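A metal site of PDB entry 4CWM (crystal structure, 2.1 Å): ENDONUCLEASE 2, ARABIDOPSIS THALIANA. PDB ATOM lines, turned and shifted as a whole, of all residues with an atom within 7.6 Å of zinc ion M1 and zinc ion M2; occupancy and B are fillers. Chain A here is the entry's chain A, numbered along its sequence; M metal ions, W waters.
The indole nitrogen (NE1) of Trp 1 is in hydrogen-bond range of the backbone carbonyl oxygen (O) of Gly 123 (2.6 Å).
The side-chain amino group (NZ) of Lys 48 lies close to the side-chain carboxylate (OD1) of Asp 45, at 3.7 Å.
A ring nitrogen (ND1) of His 120 is in hydrogen-bond range of the backbone carbonyl oxygen of Cys 41, at 2.9 Å.
The backbone NH of Trp 1 lies close to the side-chain carboxylate of Asp 158 (3.4 Å).
A ring nitrogen (ND1) of His 130 is in hydrogen-bond range of the backbone carbonyl oxygen (O) of His 58 (2.6 Å).
Of the 25 residues printed, 5 come within 4 Å of zinc ion M1.
Along chain A the residues within 4 Å of zinc ion M1 span positions 1 to 124.
The nearest printed residue that does not touch zinc ion M1 is Gly 2 (4.3 Å).
Four residues have an atom within 4 Å of zinc ion M2: Asp 45, His 58, His 120 and Asp 124.
Zinc ion M1 is bound by water W3, a ring nitrogen (NE2) of His 6, the backbone nitrogen (N) of Trp 1, the side-chain carboxylate (OD1) of Asp 124 and the backbone carbonyl oxygen (O) of Trp 1.
Zinc ion M2 is bound by water W3, 2.1 Å away.
The side-chain carboxylate (OD2) of Asp 124 binds zinc ion M2 (2.3 Å).
Zinc ion M2 is bound by a ring nitrogen (ND1) of His 58.
Zinc ion M2 is bound by NE2 of His 120, 2.4 Å away.
OD1 of Asp 45 is bound to zinc ion M2, at 2.4 Å.
Zinc ion M2 is bound by water W2.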
ATOM      1  N   TRP A   1      29.661  13.146   3.340  1.00  0.00           N
ATOM      2  CA  TRP A   1      30.986  13.551   3.881  1.00  0.00           C
ATOM      3  C   TRP A   1      32.117  13.232   2.936  1.00  0.00           C
ATOM      4  O   TRP A   1      31.995  12.404   2.035  1.00  0.00           O
ATOM      5  CB  TRP A   1      31.317  12.816   5.184  1.00  0.00           C
ATOM      6  CG  TRP A   1      30.232  12.801   6.194  1.00  0.00           C
ATOM      7  CD1 TRP A   1      29.259  11.860   6.326  1.00  0.00           C
ATOM      8  CD2 TRP A   1      30.031  13.750   7.238  1.00  0.00           C
ATOM      9  NE1 TRP A   1      28.460  12.164   7.395  1.00  0.00           N
ATOM     10  CE2 TRP A   1      28.921  13.331   7.973  1.00  0.00           C
ATOM     11  CE3 TRP A   1      30.685  14.914   7.631  1.00  0.00           C
ATOM     12  CZ2 TRP A   1      28.435  14.025   9.074  1.00  0.00           C
ATOM     13  CZ3 TRP A   1      30.218  15.623   8.733  1.00  0.00           C
ATOM     14  CH2 TRP A   1      29.099  15.174   9.430  1.00  0.00           C
ATOM     15  N   GLY A   2      33.242  13.865   3.173  1.00  0.00           N
ATOM     16  CA  GLY A   2      34.437  13.523   2.465  1.00  0.00           C
ATOM     17  C   GLY A   2      34.990  12.287   3.134  1.00  0.00           C
ATOM     18  O   GLY A   2      34.325  11.642   3.953  1.00  0.00           O
ATOM     19  N   LYS A   3      36.230  11.999   2.817  1.00  0.00           N
ATOM     20  CA  LYS A   3      36.857  10.742   3.194  1.00  0.00           C
ATOM     21  C   LYS A   3      36.985  10.514   4.682  1.00  0.00           C
ATOM     22  O   LYS A   3      36.662   9.425   5.156  1.00  0.00           O
ATOM     23  CB  LYS A   3      38.233  10.656   2.528  1.00  0.00           C
ATOM     24  CG  LYS A   3      38.990   9.394   2.887  1.00  0.00           C
ATOM     25  CD  LYS A   3      40.153   9.690   3.828  1.00  0.00           C
ATOM     26  CE  LYS A   3      41.491   9.480   3.149  1.00  0.00           C
ATOM     27  NZ  LYS A   3      41.832   8.029   3.123  1.00  0.00           N
ATOM     28  N   GLY A   5      35.253  11.785   7.203  1.00  0.00           N
ATOM     29  CA  GLY A   5      33.963  11.574   7.863  1.00  0.00           C
ATOM     30  C   GLY A   5      33.494  10.150   7.679  1.00  0.00           C
ATOM     31  O   GLY A   5      33.081   9.496   8.641  1.00  0.00           O
ATOM     32  N   HIS A   6      33.573   9.638   6.460  1.00  0.00           N
ATOM     33  CA  HIS A   6      33.147   8.257   6.193  1.00  0.00           C
ATOM     34  C   HIS A   6      34.028   7.209   6.887  1.00  0.00           C
ATOM     35  O   HIS A   6      33.541   6.152   7.323  1.00  0.00           O
ATOM     36  CB  HIS A   6      33.101   8.000   4.672  1.00  0.00           C
ATOM     37  CG  HIS A   6      31.915   8.627   3.997  1.00  0.00           C
ATOM     38  ND1 HIS A   6      30.627   8.204   4.222  1.00  0.00           N
ATOM     39  CD2 HIS A   6      31.828   9.656   3.126  1.00  0.00           C
ATOM     40  CE1 HIS A   6      29.791   8.932   3.498  1.00  0.00           C
ATOM     41  NE2 HIS A   6      30.497   9.813   2.829  1.00  0.00           N
ATOM     42  N   CYS A  41      34.500   2.695   2.329  1.00  0.00           N
ATOM     43  CA  CYS A  41      33.302   3.464   2.652  1.00  0.00           C
ATOM     44  C   CYS A  41      33.188   4.751   1.834  1.00  0.00           C
ATOM     45  O   CYS A  41      32.198   5.470   1.963  1.00  0.00           O
ATOM     46  CB  CYS A  41      33.153   3.714   4.159  1.00  0.00           C
ATOM     47  SG  CYS A  41      32.599   2.265   5.099  1.00  0.00           S
ATOM     48  N   LEU A  42      34.167   5.040   0.987  1.00  0.00           N
ATOM     49  CA  LEU A  42      34.046   6.137   0.006  1.00  0.00           C
ATOM     50  C   LEU A  42      33.755   5.615  -1.378  1.00  0.00           C
ATOM     51  O   LEU A  42      33.547   6.408  -2.281  1.00  0.00           O
ATOM     52  CB  LEU A  42      35.294   7.025  -0.022  1.00  0.00           C
ATOM     53  CG  LEU A  42      35.091   8.510  -0.308  1.00  0.00           C
ATOM     54  CD1 LEU A  42      34.292   9.244   0.785  1.00  0.00           C
ATOM     55  CD2 LEU A  42      36.451   9.147  -0.472  1.00  0.00           C
ATOM     56  N   ALA A  44      31.189   4.439  -2.903  1.00  0.00           N
ATOM     57  CA  ALA A  44      30.013   4.993  -3.553  1.00  0.00           C
ATOM     58  C   ALA A  44      30.285   6.368  -4.225  1.00  0.00           C
ATOM     59  O   ALA A  44      29.665   6.707  -5.229  1.00  0.00           O
ATOM     60  CB  ALA A  44      28.888   5.112  -2.546  1.00  0.00           C
ATOM     61  N   ASP A  45      31.224   7.150  -3.698  1.00  0.00           N
ATOM     62  CA  ASP A  45      31.476   8.478  -4.291  1.00  0.00           C
ATOM     63  C   ASP A  45      32.215   8.348  -5.639  1.00  0.00           C
ATOM     64  O   ASP A  45      32.258   9.295  -6.421  1.00  0.00           O
ATOM     65  CB  ASP A  45      32.250   9.396  -3.343  1.00  0.00           C
ATOM     66  CG  ASP A  45      31.346  10.154  -2.345  1.00  0.00           C
ATOM     67  OD1 ASP A  45      30.135  10.378  -2.598  1.00  0.00           O
ATOM     68  OD2 ASP A  45      31.888  10.548  -1.292  1.00  0.00           O
ATOM     69  N   ARG A  46      32.805   7.176  -5.889  1.00  0.00           N
ATOM     70  CA  ARG A  46      33.589   6.914  -7.098  1.00  0.00           C
ATOM     71  C   ARG A  46      32.741   6.342  -8.214  1.00  0.00           C
ATOM     72  O   ARG A  46      33.222   6.233  -9.324  1.00  0.00           O
ATOM     73  CB  ARG A  46      34.723   5.910  -6.809  1.00  0.00           C
ATOM     74  CG  ARG A  46      35.703   6.370  -5.750  1.00  0.00           C
ATOM     75  CD  ARG A  46      36.845   5.387  -5.537  1.00  0.00           C
ATOM     76  NE  ARG A  46      36.597   4.369  -4.501  1.00  0.00           N
ATOM     77  CZ  ARG A  46      37.018   4.431  -3.240  1.00  0.00           C
ATOM     78  NH1 ARG A  46      37.720   5.477  -2.797  1.00  0.00           N
ATOM     79  NH2 ARG A  46      36.745   3.422  -2.409  1.00  0.00           N
ATOM     80  N   LYS A  48      29.461   7.580  -9.116  1.00  0.00           N
ATOM     81  CA  LYS A  48      28.344   8.459  -9.496  1.00  0.00           C
ATOM     82  C   LYS A  48      28.079   8.568 -11.014  1.00  0.00           C
ATOM     83  O   LYS A  48      26.976   8.854 -11.416  1.00  0.00           O
ATOM     84  CB  LYS A  48      28.526   9.877  -8.936  1.00  0.00           C
ATOM     85  CG  LYS A  48      28.598   9.942  -7.416  1.00  0.00           C
ATOM     86  CD  LYS A  48      28.576  11.375  -6.934  1.00  0.00           C
ATOM     87  CE  LYS A  48      28.608  11.463  -5.442  1.00  0.00           C
ATOM     88  NZ  LYS A  48      28.875  12.881  -5.055  1.00  0.00           N
ATOM     89  N   SER A  55      23.601   8.810  -8.351  1.00  0.00           N
ATOM     90  CA  SER A  55      24.080  10.087  -7.847  1.00  0.00           C
ATOM     91  C   SER A  55      23.070  10.871  -7.005  1.00  0.00           C
ATOM     92  O   SER A  55      23.462  11.522  -6.024  1.00  0.00           O
ATOM     93  CB  SER A  55      24.763  10.964  -8.935  1.00  0.00           C
ATOM     94  OG  SER A  55      23.890  11.403  -9.949  1.00  0.00           O
ATOM     95  N   LEU A  57      21.253   9.555  -4.920  1.00  0.00           N
ATOM     96  CA  LEU A  57      21.060   8.694  -3.775  1.00  0.00           C
ATOM     97  C   LEU A  57      21.933   9.125  -2.623  1.00  0.00           C
ATOM     98  O   LEU A  57      21.838   8.564  -1.540  1.00  0.00           O
ATOM     99  CB  LEU A  57      21.382   7.231  -4.115  1.00  0.00           C
ATOM    100  CG  LEU A  57      20.605   6.621  -5.289  1.00  0.00           C
ATOM    101  CD1 LEU A  57      20.994   5.193  -5.593  1.00  0.00           C
ATOM    102  CD2 LEU A  57      19.094   6.707  -5.038  1.00  0.00           C
ATOM    103  N   HIS A  58      22.789  10.108  -2.875  1.00  0.00           N
ATOM    104  CA  HIS A  58      23.701  10.588  -1.851  1.00  0.00           C
ATOM    105  C   HIS A  58      23.090  11.672  -0.947  1.00  0.00           C
ATOM    106  O   HIS A  58      23.682  12.023   0.048  1.00  0.00           O
ATOM    107  CB  HIS A  58      24.957  11.113  -2.490  1.00  0.00           C
ATOM    108  CG  HIS A  58      25.810  10.047  -3.101  1.00  0.00           C
ATOM    109  ND1 HIS A  58      26.998   9.649  -2.560  1.00  0.00           N
ATOM    110  CD2 HIS A  58      25.633   9.288  -4.208  1.00  0.00           C
ATOM    111  CE1 HIS A  58      27.530   8.678  -3.296  1.00  0.00           C
ATOM    112  NE2 HIS A  58      26.712   8.445  -4.304  1.00  0.00           N
ATOM    113  N   TYR A  59      21.918  12.205  -1.293  1.00  0.00           N
ATOM    114  CA  TYR A  59      21.385  13.399  -0.593  1.00  0.00           C
ATOM    115  C   TYR A  59      19.869  13.490  -0.662  1.00  0.00           C
ATOM    116  O   TYR A  59      19.238  12.661  -1.279  1.00  0.00           O
ATOM    117  CB  TYR A  59      21.994  14.690  -1.185  1.00  0.00           C
ATOM    118  CG  TYR A  59      21.735  14.799  -2.671  1.00  0.00           C
ATOM    119  CD1 TYR A  59      20.538  15.353  -3.168  1.00  0.00           C
ATOM    120  CD2 TYR A  59      22.653  14.276  -3.587  1.00  0.00           C
ATOM    121  CE1 TYR A  59      20.305  15.445  -4.539  1.00  0.00           C
ATOM    122  CE2 TYR A  59      22.428  14.356  -4.954  1.00  0.00           C
ATOM    123  CZ  TYR A  59      21.252  14.927  -5.425  1.00  0.00           C
ATOM    124  OH  TYR A  59      21.070  14.949  -6.785  1.00  0.00           O
ATOM    125  N   VAL A  85      18.763   9.644  -0.582  1.00  0.00           N
ATOM    126  CA  VAL A  85      19.557   8.895   0.392  1.00  0.00           C
ATOM    127  C   VAL A  85      18.699   8.045   1.336  1.00  0.00           C
ATOM    128  O   VAL A  85      19.070   6.938   1.654  1.00  0.00           O
ATOM    129  CB  VAL A  85      20.580   9.783   1.145  1.00  0.00           C
ATOM    130  CG1 VAL A  85      19.879  10.707   2.151  1.00  0.00           C
ATOM    131  CG2 VAL A  85      21.574   8.912   1.850  1.00  0.00           C
ATOM    132  N   HIS A 120      27.963   3.767   3.035  1.00  0.00           N
ATOM    133  CA  HIS A 120      28.181   5.139   2.588  1.00  0.00           C
ATOM    134  C   HIS A 120      26.991   6.038   2.837  1.00  0.00           C
ATOM    135  O   HIS A 120      27.129   7.142   3.329  1.00  0.00           O
ATOM    136  CB  HIS A 120      28.492   5.131   1.122  1.00  0.00           C
ATOM    137  CG  HIS A 120      28.861   6.476   0.612  1.00  0.00           C
ATOM    138  ND1 HIS A 120      30.123   6.997   0.739  1.00  0.00           N
ATOM    139  CD2 HIS A 120      28.126   7.409  -0.012  1.00  0.00           C
ATOM    140  CE1 HIS A 120      30.153   8.198   0.198  1.00  0.00           C
ATOM    141  NE2 HIS A 120      28.942   8.483  -0.240  1.00  0.00           N
ATOM    142  N   PHE A 121      25.792   5.540   2.496  1.00  0.00           N
ATOM    143  CA  PHE A 121      24.604   6.340   2.609  1.00  0.00           C
ATOM    144  C   PHE A 121      24.194   6.603   4.066  1.00  0.00           C
ATOM    145  O   PHE A 121      23.696   7.698   4.370  1.00  0.00           O
ATOM    146  CB  PHE A 121      23.479   5.717   1.789  1.00  0.00           C
ATOM    147  CG  PHE A 121      23.765   5.671   0.295  1.00  0.00           C
ATOM    148  CD1 PHE A 121      24.532   6.669  -0.327  1.00  0.00           C
ATOM    149  CD2 PHE A 121      23.269   4.633  -0.491  1.00  0.00           C
ATOM    150  CE1 PHE A 121      24.800   6.605  -1.676  1.00  0.00           C
ATOM    151  CE2 PHE A 121      23.514   4.587  -1.844  1.00  0.00           C
ATOM    152  CZ  PHE A 121      24.285   5.578  -2.445  1.00  0.00           C
ATOM    153  N   GLY A 123      26.284   7.121   6.360  1.00  0.00           N
ATOM    154  CA  GLY A 123      27.121   8.262   6.643  1.00  0.00           C
ATOM    155  C   GLY A 123      26.583   9.569   6.053  1.00  0.00           C
ATOM    156  O   GLY A 123      26.508  10.570   6.760  1.00  0.00           O
ATOM    157  N   ASP A 124      26.219   9.534   4.783  1.00  0.00           N
ATOM    158  CA  ASP A 124      25.731  10.736   4.072  1.00  0.00           C
ATOM    159  C   ASP A 124      24.451  11.259   4.633  1.00  0.00           C
ATOM    160  O   ASP A 124      24.345  12.454   4.722  1.00  0.00           O
ATOM    161  CB  ASP A 124      25.542  10.524   2.575  1.00  0.00           C
ATOM    162  CG  ASP A 124      26.786  10.822   1.780  1.00  0.00           C
ATOM    163  OD1 ASP A 124      27.806  11.127   2.364  1.00  0.00           O
ATOM    164  OD2 ASP A 124      26.742  10.709   0.565  1.00  0.00           O
ATOM    165  N   ILE A 125      23.494  10.397   5.022  1.00  0.00           N
ATOM    166  CA  ILE A 125      22.224  10.871   5.603  1.00  0.00           C
ATOM    167  C   ILE A 125      22.411  11.629   6.915  1.00  0.00           C
ATOM    168  O   ILE A 125      21.513  12.338   7.400  1.00  0.00           O
ATOM    169  CB  ILE A 125      21.169   9.736   5.760  1.00  0.00           C
ATOM    170  CG1 ILE A 125      19.758  10.330   5.758  1.00  0.00           C
ATOM    171  CG2 ILE A 125      21.407   8.924   7.036  1.00  0.00           C
ATOM    172  CD1 ILE A 125      18.613   9.333   5.514  1.00  0.00           C
ATOM    173  N   GLN A 127      25.146  13.764   7.310  1.00  0.00           N
ATOM    174  CA  GLN A 127      25.670  15.082   6.933  1.00  0.00           C
ATOM    175  C   GLN A 127      24.493  16.068   6.832  1.00  0.00           C
ATOM    176  O   GLN A 127      23.597  15.878   6.000  1.00  0.00           O
ATOM    177  CB  GLN A 127      26.448  15.021   5.599  1.00  0.00           C
ATOM    178  CG  GLN A 127      27.724  15.902   5.550  1.00  0.00           C
ATOM    179  CD  GLN A 127      27.446  17.373   5.338  1.00  0.00           C
ATOM    180  OE1 GLN A 127      26.713  18.016   6.090  1.00  0.00           O
ATOM    181  NE2 GLN A 127      28.069  17.933   4.319  1.00  0.00           N
ATOM    182  N   HIS A 130      23.634  17.237   3.449  1.00  0.00           N
ATOM    183  CA  HIS A 130      23.162  16.232   2.454  1.00  0.00           C
ATOM    184  C   HIS A 130      21.652  16.047   2.555  1.00  0.00           C
ATOM    185  O   HIS A 130      21.071  15.195   1.834  1.00  0.00           O
ATOM    186  CB  HIS A 130      23.839  14.882   2.651  1.00  0.00           C
ATOM    187  CG  HIS A 130      25.128  14.762   1.938  1.00  0.00           C
ATOM    188  ND1 HIS A 130      25.297  13.941   0.859  1.00  0.00           N
ATOM    189  CD2 HIS A 130      26.298  15.428   2.089  1.00  0.00           C
ATOM    190  CE1 HIS A 130      26.523  14.103   0.368  1.00  0.00           C
ATOM    191  NE2 HIS A 130      27.160  14.980   1.117  1.00  0.00           N
ATOM    192  N   HIS A 154      28.958  23.689   1.757  1.00  0.00           N
ATOM    193  CA  HIS A 154      28.744  22.260   1.765  1.00  0.00           C
ATOM    194  C   HIS A 154      30.060  21.582   2.089  1.00  0.00           C
ATOM    195  O   HIS A 154      30.113  20.690   2.929  1.00  0.00           O
ATOM    196  CB  HIS A 154      28.247  21.771   0.398  1.00  0.00           C
ATOM    197  CG  HIS A 154      27.951  20.319   0.358  1.00  0.00           C
ATOM    198  ND1 HIS A 154      26.718  19.813   0.712  1.00  0.00           N
ATOM    199  CD2 HIS A 154      28.727  19.262   0.067  1.00  0.00           C
ATOM    200  CE1 HIS A 154      26.762  18.494   0.651  1.00  0.00           C
ATOM    201  NE2 HIS A 154      27.975  18.135   0.275  1.00  0.00           N
ATOM    202  N   ASP A 158      31.359  18.767   4.745  1.00  0.00           N
ATOM    203  CA  ASP A 158      31.913  17.469   4.292  1.00  0.00           C
ATOM    204  C   ASP A 158      33.281  17.173   4.879  1.00  0.00           C
ATOM    205  O   ASP A 158      33.524  16.059   5.335  1.00  0.00           O
ATOM    206  CB  ASP A 158      32.043  17.429   2.773  1.00  0.00           C
ATOM    207  CG  ASP A 158      30.779  16.999   2.083  1.00  0.00           C
ATOM    208  OD1 ASP A 158      29.871  16.523   2.775  1.00  0.00           O
ATOM    209  OD2 ASP A 158      30.700  17.101   0.830  1.00  0.00           O
HETATM  210 ZN    ZN M   1      29.847  11.596   1.943  1.00  0.00          ZN
HETATM  211 ZN    ZN M   2      28.362  10.640  -1.027  1.00  0.00          ZN
HETATM  212 ZN    ZN M   3      28.784  16.204   0.405  1.00  0.00          ZN
HETATM  213  O   HOH W   1      29.847  14.386   0.121  1.00  0.00           O
HETATM  214  O   HOH W   2      27.977  12.659  -2.270  1.00  0.00           O
HETATM  215  O   HOH W   3      29.840  11.833  -0.051  1.00  0.00           O
